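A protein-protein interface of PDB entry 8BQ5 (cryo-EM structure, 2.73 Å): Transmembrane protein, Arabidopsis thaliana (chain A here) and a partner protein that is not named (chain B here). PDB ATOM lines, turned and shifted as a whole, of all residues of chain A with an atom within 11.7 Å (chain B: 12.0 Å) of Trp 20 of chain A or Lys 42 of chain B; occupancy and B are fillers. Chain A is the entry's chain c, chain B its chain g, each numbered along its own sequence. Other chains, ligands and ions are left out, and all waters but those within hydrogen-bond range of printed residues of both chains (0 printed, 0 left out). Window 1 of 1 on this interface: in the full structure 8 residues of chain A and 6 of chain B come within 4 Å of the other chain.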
ATOM      1  N   GLY A  13       6.357  -8.647  -2.148  1.00  0.00           N
ATOM      2  CA  GLY A  13       5.798  -9.962  -1.897  1.00  0.00           C
ATOM      3  C   GLY A  13       5.567 -10.232  -0.423  1.00  0.00           C
ATOM      4  O   GLY A  13       4.635  -9.695   0.175  1.00  0.00           O
ATOM      5  N   ASP A  14       6.415 -11.074   0.163  1.00  0.00           N
ATOM      6  CA  ASP A  14       6.365 -11.369   1.588  1.00  0.00           C
ATOM      7  C   ASP A  14       7.595 -10.878   2.334  1.00  0.00           C
ATOM      8  O   ASP A  14       7.472 -10.091   3.276  1.00  0.00           O
ATOM      9  CB  ASP A  14       6.191 -12.878   1.806  1.00  0.00           C
ATOM     10  CG  ASP A  14       4.811 -13.366   1.423  1.00  0.00           C
ATOM     11  OD1 ASP A  14       3.904 -12.523   1.261  1.00  0.00           O
ATOM     12  OD2 ASP A  14       4.632 -14.592   1.277  1.00  0.00           O
ATOM     13  N   PHE A  15       8.790 -11.318   1.933  1.00  0.00           N
ATOM     14  CA  PHE A  15       9.999 -10.850   2.600  1.00  0.00           C
ATOM     15  C   PHE A  15      10.358  -9.428   2.192  1.00  0.00           C
ATOM     16  O   PHE A  15      10.990  -8.707   2.970  1.00  0.00           O
ATOM     17  CB  PHE A  15      11.166 -11.807   2.330  1.00  0.00           C
ATOM     18  CG  PHE A  15      11.708 -11.745   0.927  1.00  0.00           C
ATOM     19  CD1 PHE A  15      12.687 -10.825   0.580  1.00  0.00           C
ATOM     20  CD2 PHE A  15      11.252 -12.622  -0.039  1.00  0.00           C
ATOM     21  CE1 PHE A  15      13.184 -10.774  -0.706  1.00  0.00           C
ATOM     22  CE2 PHE A  15      11.750 -12.576  -1.324  1.00  0.00           C
ATOM     23  CZ  PHE A  15      12.715 -11.650  -1.657  1.00  0.00           C
ATOM     24  N   ARG A  16       9.961  -9.006   0.989  1.00  0.00           N
ATOM     25  CA  ARG A  16      10.266  -7.653   0.540  1.00  0.00           C
ATOM     26  C   ARG A  16       9.600  -6.593   1.407  1.00  0.00           C
ATOM     27  O   ARG A  16      10.026  -5.434   1.383  1.00  0.00           O
ATOM     28  CB  ARG A  16       9.858  -7.483  -0.924  1.00  0.00           C
ATOM     29  CG  ARG A  16      10.382  -8.589  -1.826  1.00  0.00           C
ATOM     30  CD  ARG A  16      10.241  -8.238  -3.293  1.00  0.00           C
ATOM     31  NE  ARG A  16       8.878  -8.432  -3.772  1.00  0.00           N
ATOM     32  CZ  ARG A  16       8.563  -8.783  -5.010  1.00  0.00           C
ATOM     33  NH1 ARG A  16       9.493  -9.003  -5.925  1.00  0.00           N
ATOM     34  NH2 ARG A  16       7.282  -8.926  -5.337  1.00  0.00           N
ATOM     35  N   ALA A  17       8.573  -6.964   2.173  1.00  0.00           N
ATOM     36  CA  ALA A  17       7.978  -6.052   3.141  1.00  0.00           C
ATOM     37  C   ALA A  17       8.891  -5.779   4.328  1.00  0.00           C
ATOM     38  O   ALA A  17       8.672  -4.795   5.043  1.00  0.00           O
ATOM     39  CB  ALA A  17       6.643  -6.608   3.634  1.00  0.00           C
ATOM     40  N   LYS A  18       9.898  -6.618   4.560  1.00  0.00           N
ATOM     41  CA  LYS A  18      10.884  -6.384   5.603  1.00  0.00           C
ATOM     42  C   LYS A  18      12.198  -5.854   5.048  1.00  0.00           C
ATOM     43  O   LYS A  18      13.210  -5.869   5.755  1.00  0.00           O
ATOM     44  CB  LYS A  18      11.129  -7.665   6.404  1.00  0.00           C
ATOM     45  CG  LYS A  18       9.863  -8.427   6.763  1.00  0.00           C
ATOM     46  CD  LYS A  18       9.962  -9.085   8.138  1.00  0.00           C
ATOM     47  CE  LYS A  18      11.368  -9.583   8.450  1.00  0.00           C
ATOM     48  NZ  LYS A  18      11.589 -10.969   7.953  1.00  0.00           N
ATOM     49  N   VAL A  19      12.206  -5.386   3.803  1.00  0.00           N
ATOM     50  CA  VAL A  19      13.411  -4.897   3.147  1.00  0.00           C
ATOM     51  C   VAL A  19      13.266  -3.396   2.942  1.00  0.00           C
ATOM     52  O   VAL A  19      12.295  -2.936   2.326  1.00  0.00           O
ATOM     53  CB  VAL A  19      13.662  -5.614   1.812  1.00  0.00           C
ATOM     54  CG1 VAL A  19      14.731  -4.886   1.015  1.00  0.00           C
ATOM     55  CG2 VAL A  19      14.058  -7.060   2.052  1.00  0.00           C
ATOM     56  N   TRP A  20      14.231  -2.640   3.450  1.00  0.00           N
ATOM     57  CA  TRP A  20      14.257  -1.192   3.302  1.00  0.00           C
ATOM     58  C   TRP A  20      15.037  -0.816   2.050  1.00  0.00           C
ATOM     59  O   TRP A  20      16.145  -1.313   1.830  1.00  0.00           O
ATOM     60  CB  TRP A  20      14.894  -0.549   4.534  1.00  0.00           C
ATOM     61  CG  TRP A  20      14.759   0.940   4.613  1.00  0.00           C
ATOM     62  CD1 TRP A  20      13.825   1.639   5.316  1.00  0.00           C
ATOM     63  CD2 TRP A  20      15.603   1.916   3.986  1.00  0.00           C
ATOM     64  NE1 TRP A  20      14.025   2.989   5.158  1.00  0.00           N
ATOM     65  CE2 TRP A  20      15.111   3.185   4.348  1.00  0.00           C
ATOM     66  CE3 TRP A  20      16.723   1.840   3.152  1.00  0.00           C
ATOM     67  CZ2 TRP A  20      15.701   4.367   3.905  1.00  0.00           C
ATOM     68  CZ3 TRP A  20      17.305   3.014   2.713  1.00  0.00           C
ATOM     69  CH2 TRP A  20      16.791   4.261   3.088  1.00  0.00           C
ATOM     70  N   SER A  21      14.453   0.056   1.231  1.00  0.00           N
ATOM     71  CA  SER A  21      15.138   0.609   0.072  1.00  0.00           C
ATOM     72  C   SER A  21      14.808   2.091  -0.033  1.00  0.00           C
ATOM     73  O   SER A  21      13.803   2.563   0.502  1.00  0.00           O
ATOM     74  CB  SER A  21      14.754  -0.112  -1.227  1.00  0.00           C
ATOM     75  OG  SER A  21      13.359  -0.045  -1.458  1.00  0.00           O
ATOM     76  N   MET A  22      15.684   2.827  -0.717  1.00  0.00           N
ATOM     77  CA  MET A  22      15.460   4.259  -0.887  1.00  0.00           C
ATOM     78  C   MET A  22      14.364   4.529  -1.906  1.00  0.00           C
ATOM     79  O   MET A  22      13.623   5.511  -1.785  1.00  0.00           O
ATOM     80  CB  MET A  22      16.756   4.946  -1.307  1.00  0.00           C
ATOM     81  CG  MET A  22      18.007   4.172  -0.958  1.00  0.00           C
ATOM     82  SD  MET A  22      19.484   4.952  -1.626  1.00  0.00           S
ATOM     83  CE  MET A  22      19.445   6.512  -0.752  1.00  0.00           C
ATOM     84  N   THR A  23      14.251   3.674  -2.918  1.00  0.00           N
ATOM     85  CA  THR A  23      13.269   3.870  -3.973  1.00  0.00           C
ATOM     86  C   THR A  23      11.880   3.387  -3.577  1.00  0.00           C
ATOM     87  O   THR A  23      10.916   3.653  -4.302  1.00  0.00           O
ATOM     88  CB  THR A  23      13.736   3.156  -5.241  1.00  0.00           C
ATOM     89  OG1 THR A  23      15.163   3.229  -5.317  1.00  0.00           O
ATOM     90  CG2 THR A  23      13.162   3.828  -6.467  1.00  0.00           C
ATOM     91  N   GLY A  24      11.753   2.696  -2.447  1.00  0.00           N
ATOM     92  CA  GLY A  24      10.467   2.309  -1.915  1.00  0.00           C
ATOM     93  C   GLY A  24      10.135   0.839  -2.029  1.00  0.00           C
ATOM     94  O   GLY A  24       9.334   0.342  -1.229  1.00  0.00           O
ATOM     95  N   GLY A  25      10.723   0.128  -2.985  1.00  0.00           N
ATOM     96  CA  GLY A  25      10.437  -1.272  -3.169  1.00  0.00           C
ATOM     97  C   GLY A  25       9.234  -1.503  -4.060  1.00  0.00           C
ATOM     98  O   GLY A  25       8.708  -0.580  -4.688  1.00  0.00           O
ATOM     99  N   PRO A  26       8.776  -2.750  -4.132  1.00  0.00           N
ATOM    100  CA  PRO A  26       7.641  -3.069  -5.004  1.00  0.00           C
ATOM    101  C   PRO A  26       6.323  -2.611  -4.402  1.00  0.00           C
ATOM    102  O   PRO A  26       6.031  -2.862  -3.230  1.00  0.00           O
ATOM    103  CB  PRO A  26       7.699  -4.597  -5.115  1.00  0.00           C
ATOM    104  CG  PRO A  26       8.382  -5.045  -3.863  1.00  0.00           C
ATOM    105  CD  PRO A  26       9.235  -3.914  -3.355  1.00  0.00           C
ATOM    106  N   ASN A  27       5.525  -1.931  -5.230  1.00  0.00           N
ATOM    107  CA  ASN A  27       4.196  -1.451  -4.849  1.00  0.00           C
ATOM    108  C   ASN A  27       4.267  -0.500  -3.654  1.00  0.00           C
ATOM    109  O   ASN A  27       3.707  -0.759  -2.589  1.00  0.00           O
ATOM    110  CB  ASN A  27       3.254  -2.621  -4.555  1.00  0.00           C
ATOM    111  CG  ASN A  27       3.126  -3.573  -5.723  1.00  0.00           C
ATOM    112  OD1 ASN A  27       2.798  -3.169  -6.837  1.00  0.00           O
ATOM    113  ND2 ASN A  27       3.387  -4.851  -5.472  1.00  0.00           N
ATOM    114  N   CYS A  28       4.959   0.620  -3.842  1.00  0.00           N
ATOM    115  CA  CYS A  28       5.095   1.609  -2.782  1.00  0.00           C
ATOM    116  C   CYS A  28       3.907   2.564  -2.820  1.00  0.00           C
ATOM    117  O   CYS A  28       3.680   3.242  -3.827  1.00  0.00           O
ATOM    118  CB  CYS A  28       6.408   2.373  -2.928  1.00  0.00           C
ATOM    119  SG  CYS A  28       6.833   3.397  -1.504  1.00  0.00           S
ATOM    120  N   ARG A  29       3.148   2.610  -1.727  1.00  0.00           N
ATOM    121  CA  ARG A  29       1.973   3.472  -1.599  1.00  0.00           C
ATOM    122  C   ARG A  29       2.001   4.175  -0.249  1.00  0.00           C
ATOM    123  O   ARG A  29       1.210   3.853   0.645  1.00  0.00           O
ATOM    124  CB  ARG A  29       0.686   2.661  -1.750  1.00  0.00           C
ATOM    125  CG  ARG A  29       0.523   1.955  -3.081  1.00  0.00           C
ATOM    126  CD  ARG A  29      -0.126   2.852  -4.120  1.00  0.00           C
ATOM    127  NE  ARG A  29      -1.220   3.640  -3.565  1.00  0.00           N
ATOM    128  CZ  ARG A  29      -2.099   4.316  -4.293  1.00  0.00           C
ATOM    129  NH1 ARG A  29      -2.074   4.279  -5.615  1.00  0.00           N
ATOM    130  NH2 ARG A  29      -3.030   5.041  -3.681  1.00  0.00           N
ATOM    131  N   PRO A  30       2.908   5.134  -0.056  1.00  0.00           N
ATOM    132  CA  PRO A  30       2.956   5.839   1.231  1.00  0.00           C
ATOM    133  C   PRO A  30       1.652   6.573   1.506  1.00  0.00           C
ATOM    134  O   PRO A  30       1.017   7.115   0.600  1.00  0.00           O
ATOM    135  CB  PRO A  30       4.133   6.808   1.069  1.00  0.00           C
ATOM    136  CG  PRO A  30       4.372   6.901  -0.391  1.00  0.00           C
ATOM    137  CD  PRO A  30       3.955   5.597  -0.980  1.00  0.00           C
ATOM    138  N   LYS A  31       1.252   6.577   2.781  1.00  0.00           N
ATOM    139  CA  LYS A  31      -0.041   7.143   3.152  1.00  0.00           C
ATOM    140  C   LYS A  31      -0.108   8.636   2.849  1.00  0.00           C
ATOM    141  O   LYS A  31      -1.126   9.126   2.347  1.00  0.00           O
ATOM    142  CB  LYS A  31      -0.321   6.879   4.631  1.00  0.00           C
ATOM    143  CG  LYS A  31      -1.445   7.719   5.210  1.00  0.00           C
ATOM    144  CD  LYS A  31      -2.808   7.167   4.827  1.00  0.00           C
ATOM    145  CE  LYS A  31      -3.747   7.142   6.022  1.00  0.00           C
ATOM    146  NZ  LYS A  31      -5.063   6.533   5.688  1.00  0.00           N
ATOM    147  N   ARG B  40       3.598   3.100   7.703  1.00  0.00           N
ATOM    148  CA  ARG B  40       5.029   3.145   7.945  1.00  0.00           C
ATOM    149  C   ARG B  40       5.745   2.435   6.808  1.00  0.00           C
ATOM    150  O   ARG B  40       5.177   1.538   6.176  1.00  0.00           O
ATOM    151  CB  ARG B  40       5.399   2.483   9.282  1.00  0.00           C
ATOM    152  CG  ARG B  40       4.955   3.245  10.525  1.00  0.00           C
ATOM    153  CD  ARG B  40       5.420   2.533  11.790  1.00  0.00           C
ATOM    154  NE  ARG B  40       5.050   3.244  13.010  1.00  0.00           N
ATOM    155  CZ  ARG B  40       5.231   2.770  14.236  1.00  0.00           C
ATOM    156  NH1 ARG B  40       5.765   1.578  14.445  1.00  0.00           N
ATOM    157  NH2 ARG B  40       4.867   3.512  15.278  1.00  0.00           N
ATOM    158  N   PRO B  41       6.986   2.817   6.521  1.00  0.00           N
ATOM    159  CA  PRO B  41       7.729   2.177   5.430  1.00  0.00           C
ATOM    160  C   PRO B  41       7.910   0.683   5.664  1.00  0.00           C
ATOM    161  O   PRO B  41       7.677   0.151   6.750  1.00  0.00           O
ATOM    162  CB  PRO B  41       9.071   2.910   5.452  1.00  0.00           C
ATOM    163  CG  PRO B  41       8.738   4.259   5.994  1.00  0.00           C
ATOM    164  CD  PRO B  41       7.692   4.001   7.043  1.00  0.00           C
ATOM    165  N   LYS B  42       8.327   0.000   4.602  1.00  0.00           N
ATOM    166  CA  LYS B  42       8.659  -1.413   4.699  1.00  0.00           C
ATOM    167  C   LYS B  42      10.128  -1.575   5.070  1.00  0.00           C
ATOM    168  O   LYS B  42      11.000  -0.894   4.526  1.00  0.00           O
ATOM    169  CB  LYS B  42       8.360  -2.130   3.383  1.00  0.00           C
ATOM    170  CG  LYS B  42       8.938  -1.454   2.159  1.00  0.00           C
ATOM    171  CD  LYS B  42       8.906  -2.381   0.962  1.00  0.00           C
ATOM    172  CE  LYS B  42       7.522  -2.426   0.343  1.00  0.00           C
ATOM    173  NZ  LYS B  42       7.176  -1.155  -0.351  1.00  0.00           N
ATOM    174  N   GLY B  43      10.394  -2.471   6.017  1.00  0.00           N
ATOM    175  CA  GLY B  43      11.736  -2.651   6.527  1.00  0.00           C
ATOM    176  C   GLY B  43      12.146  -1.518   7.449  1.00  0.00           C
ATOM    177  O   GLY B  43      11.368  -0.624   7.785  1.00  0.00           O
ATOM    178  N   TYR B  44      13.409  -1.562   7.864  1.00  0.00           N
ATOM    179  CA  TYR B  44      13.986  -0.535   8.717  1.00  0.00           C
ATOM    180  C   TYR B  44      15.285  -0.038   8.108  1.00  0.00           C
ATOM    181  O   TYR B  44      16.040  -0.815   7.516  1.00  0.00           O
ATOM    182  CB  TYR B  44      14.239  -1.059  10.134  1.00  0.00           C
ATOM    183  CG  TYR B  44      12.980  -1.495  10.843  1.00  0.00           C
ATOM    184  CD1 TYR B  44      12.042  -0.563  11.263  1.00  0.00           C
ATOM    185  CD2 TYR B  44      12.725  -2.837  11.081  1.00  0.00           C
ATOM    186  CE1 TYR B  44      10.888  -0.955  11.905  1.00  0.00           C
ATOM    187  CE2 TYR B  44      11.576  -3.239  11.724  1.00  0.00           C
ATOM    188  CZ  TYR B  44      10.660  -2.295  12.134  1.00  0.00           C
ATOM    189  OH  TYR B  44       9.511  -2.693  12.775  1.00  0.00           O
ATOM    190  N   PHE B  45      15.539   1.259   8.256  1.00  0.00           N
ATOM    191  CA  PHE B  45      16.766   1.848   7.738  1.00  0.00           C
ATOM    192  C   PHE B  45      17.976   1.217   8.411  1.00  0.00           C
ATOM    193  O   PHE B  45      18.114   1.271   9.637  1.00  0.00           O
ATOM    194  CB  PHE B  45      16.752   3.359   7.964  1.00  0.00           C
ATOM    195  CG  PHE B  45      17.961   4.063   7.423  1.00  0.00           C
ATOM    196  CD1 PHE B  45      18.359   3.871   6.113  1.00  0.00           C
ATOM    197  CD2 PHE B  45      18.691   4.925   8.220  1.00  0.00           C
ATOM    198  CE1 PHE B  45      19.468   4.519   5.607  1.00  0.00           C
ATOM    199  CE2 PHE B  45      19.799   5.578   7.721  1.00  0.00           C
ATOM    200  CZ  PHE B  45      20.190   5.373   6.411  1.00  0.00           C
ATOM    201  N   MET B  46      18.848   0.611   7.602  1.00  0.00           N
ATOM    202  CA  MET B  46      20.056  -0.062   8.084  1.00  0.00           C
ATOM    203  C   MET B  46      19.732  -1.215   9.030  1.00  0.00           C
ATOM    204  O   MET B  46      20.539  -1.569   9.893  1.00  0.00           O
ATOM    205  CB  MET B  46      21.024   0.933   8.734  1.00  0.00           C
ATOM    206  CG  MET B  46      21.674   1.880   7.731  1.00  0.00           C
ATOM    207  SD  MET B  46      22.285   3.430   8.419  1.00  0.00           S
ATOM    208  CE  MET B  46      22.146   3.110  10.170  1.00  0.00           C
ATOM    209  N   ASN B  47      18.542  -1.796   8.867  1.00  0.00           N
ATOM    210  CA  ASN B  47      18.168  -3.076   9.474  1.00  0.00           C
ATOM    211  C   ASN B  47      18.384  -3.104  10.984  1.00  0.00           C
ATOM    212  O   ASN B  47      18.838  -4.108  11.536  1.00  0.00           O
ATOM    213  CB  ASN B  47      18.918  -4.234   8.814  1.00  0.00           C
ATOM    214  CG  ASN B  47      18.321  -4.623   7.482  1.00  0.00           C
ATOM    215  OD1 ASN B  47      18.686  -4.080   6.441  1.00  0.00           O
ATOM    216  ND2 ASN B  47      17.410  -5.583   7.505  1.00  0.00           N
ATOM    217  N   ARG B  48      18.058  -2.013  11.668  1.00  0.00           N
ATOM    218  CA  ARG B  48      18.077  -1.969  13.122  1.00  0.00           C
ATOM    219  C   ARG B  48      16.655  -1.785  13.632  1.00  0.00           C
ATOM    220  O   ARG B  48      15.936  -0.892  13.171  1.00  0.00           O
ATOM    221  CB  ARG B  48      18.982  -0.846  13.631  1.00  0.00           C
ATOM    222  CG  ARG B  48      18.771   0.481  12.938  1.00  0.00           C
ATOM    223  CD  ARG B  48      19.379   1.615  13.737  1.00  0.00           C
ATOM    224  NE  ARG B  48      20.836   1.599  13.696  1.00  0.00           N
ATOM    225  CZ  ARG B  48      21.587   2.674  13.507  1.00  0.00           C
ATOM    226  NH1 ARG B  48      21.050   3.869  13.330  1.00  0.00           N
ATOM    227  NH2 ARG B  48      22.911   2.546  13.492  1.00  0.00           N
ATOM    228  N   THR B  49      16.245  -2.643  14.561  1.00  0.00           N
ATOM    229  CA  THR B  49      14.927  -2.513  15.156  1.00  0.00           C
ATOM    230  C   THR B  49      14.850  -1.236  15.992  1.00  0.00           C
ATOM    231  O   THR B  49      15.786  -0.907  16.725  1.00  0.00           O
ATOM    232  CB  THR B  49      14.608  -3.721  16.031  1.00  0.00           C
ATOM    233  OG1 THR B  49      15.636  -3.881  17.016  1.00  0.00           O
ATOM    234  CG2 THR B  49      14.514  -4.981  15.187  1.00  0.00           C
ATOM    235  N   PRO B  50      13.749  -0.498  15.891  1.00  0.00           N
ATOM    236  CA  PRO B  50      13.614   0.748  16.646  1.00  0.00           C
ATOM    237  C   PRO B  50      13.627   0.492  18.142  1.00  0.00           C
ATOM    238  O   PRO B  50      13.233  -0.591  18.602  1.00  0.00           O
ATOM    239  CB  PRO B  50      12.252   1.283  16.183  1.00  0.00           C
ATOM    240  CG  PRO B  50      12.147   0.767  14.787  1.00  0.00           C
ATOM    241  CD  PRO B  50      12.657  -0.647  14.915  1.00  0.00           C
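The backbone carbonyl oxygen of Ala 17 of chain A lies within hydrogen-bond range of the backbone NH of Gly 43 of chain B (3.1 Å).
The backbone carbonyl oxygen of Val 19 of chain A sits close to the backbone carbonyl oxygen of Lys 42 of chain B (3.3 Å).
O of Gly 24 of chain A is in hydrogen-bond range of NZ of Lys 42 of chain B (2.8 Å).
The side-chain hydroxyl of Ser 21 of chain A is in hydrogen-bond range of the backbone NH of Gly 24 of chain A, at 3.3 Å.
Among the printed residues, pairs that only touch across the chains: Arg 16 of chain A with Lys 42 of chain B (3.3 Å), Ala 17 of chain A with Lys 42 of chain B (3.2 Å), Lys 18 of chain A with Gly 43 of chain B (3.6 Å), Val 19 of chain A with Gly 43 of chain B (3.9 Å), Trp 20 of chain A with Lys 42 of chain B (3.5 Å), Trp 20 of chain A with Gly 43 of chain B (3.96 Å), Trp 20 of chain A with Tyr 44 of chain B (3.2 Å), Trp 20 of chain A with Phe 45 of chain B (3.4 Å) and Pro 26 of chain A with Lys 42 of chain B (3.5 Å).
Of chain B, only Lys 42, Gly 43, Tyr 44 and Phe 45 come within 4 Å of Trp 20 of chain A.
Lys 42 of chain B touches six residues of chain A.
No residue of chain B comes within 4 Å of Ser 21 of chain A.
No residue of chain B comes within 4 Å of Met 22 of chain A.
No residue of chain B comes within 4 Å of Gly 25 of chain A.
Pro 26 of chain A touches just one residue of chain B: Lys 42 (3.5 Å).
Cys 28 of chain A touches none of the printed residues of chain B.
No residue of chain A comes within 4 Å of Pro 41 of chain B.
Gly 43 of chain B touches just these residues of chain A: Ala 17, Lys 18, Val 19 and Trp 20.
Phe 45 of chain B touches one residue of chain A.
Of the printed residues of chain B, Arg 16 of chain A touches Lys 42 (3.3 Å).
Of the printed residues of chain B, Lys 18 of chain A touches Gly 43.
Of the printed residues of chain A, Tyr 44 of chain B touches Trp 20 (3.2 Å).
Thr 23 of chain A touches none of the printed residues of chain B.
The nearest residue of chain A that does not touch Lys 42 of chain B is Asn 27 of chain A (4.1 Å).
Hydrophobic or aromatic side chains of chain B that line the printed part of chain A: Phe 45.
Printed residues of chain A that touch a printed residue of chain B: Arg 16, Ala 17, Lys 18, Val 19, Trp 20, Gly 24 and Pro 26.
Hydrophobic or aromatic side chains of chain A within 4 Å of the printed part of chain B: Trp 20.
Among the printed residues, no Asp or Glu carboxylate lies within 4 Å of a Lys or Arg side-chain nitrogen of the other chain.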
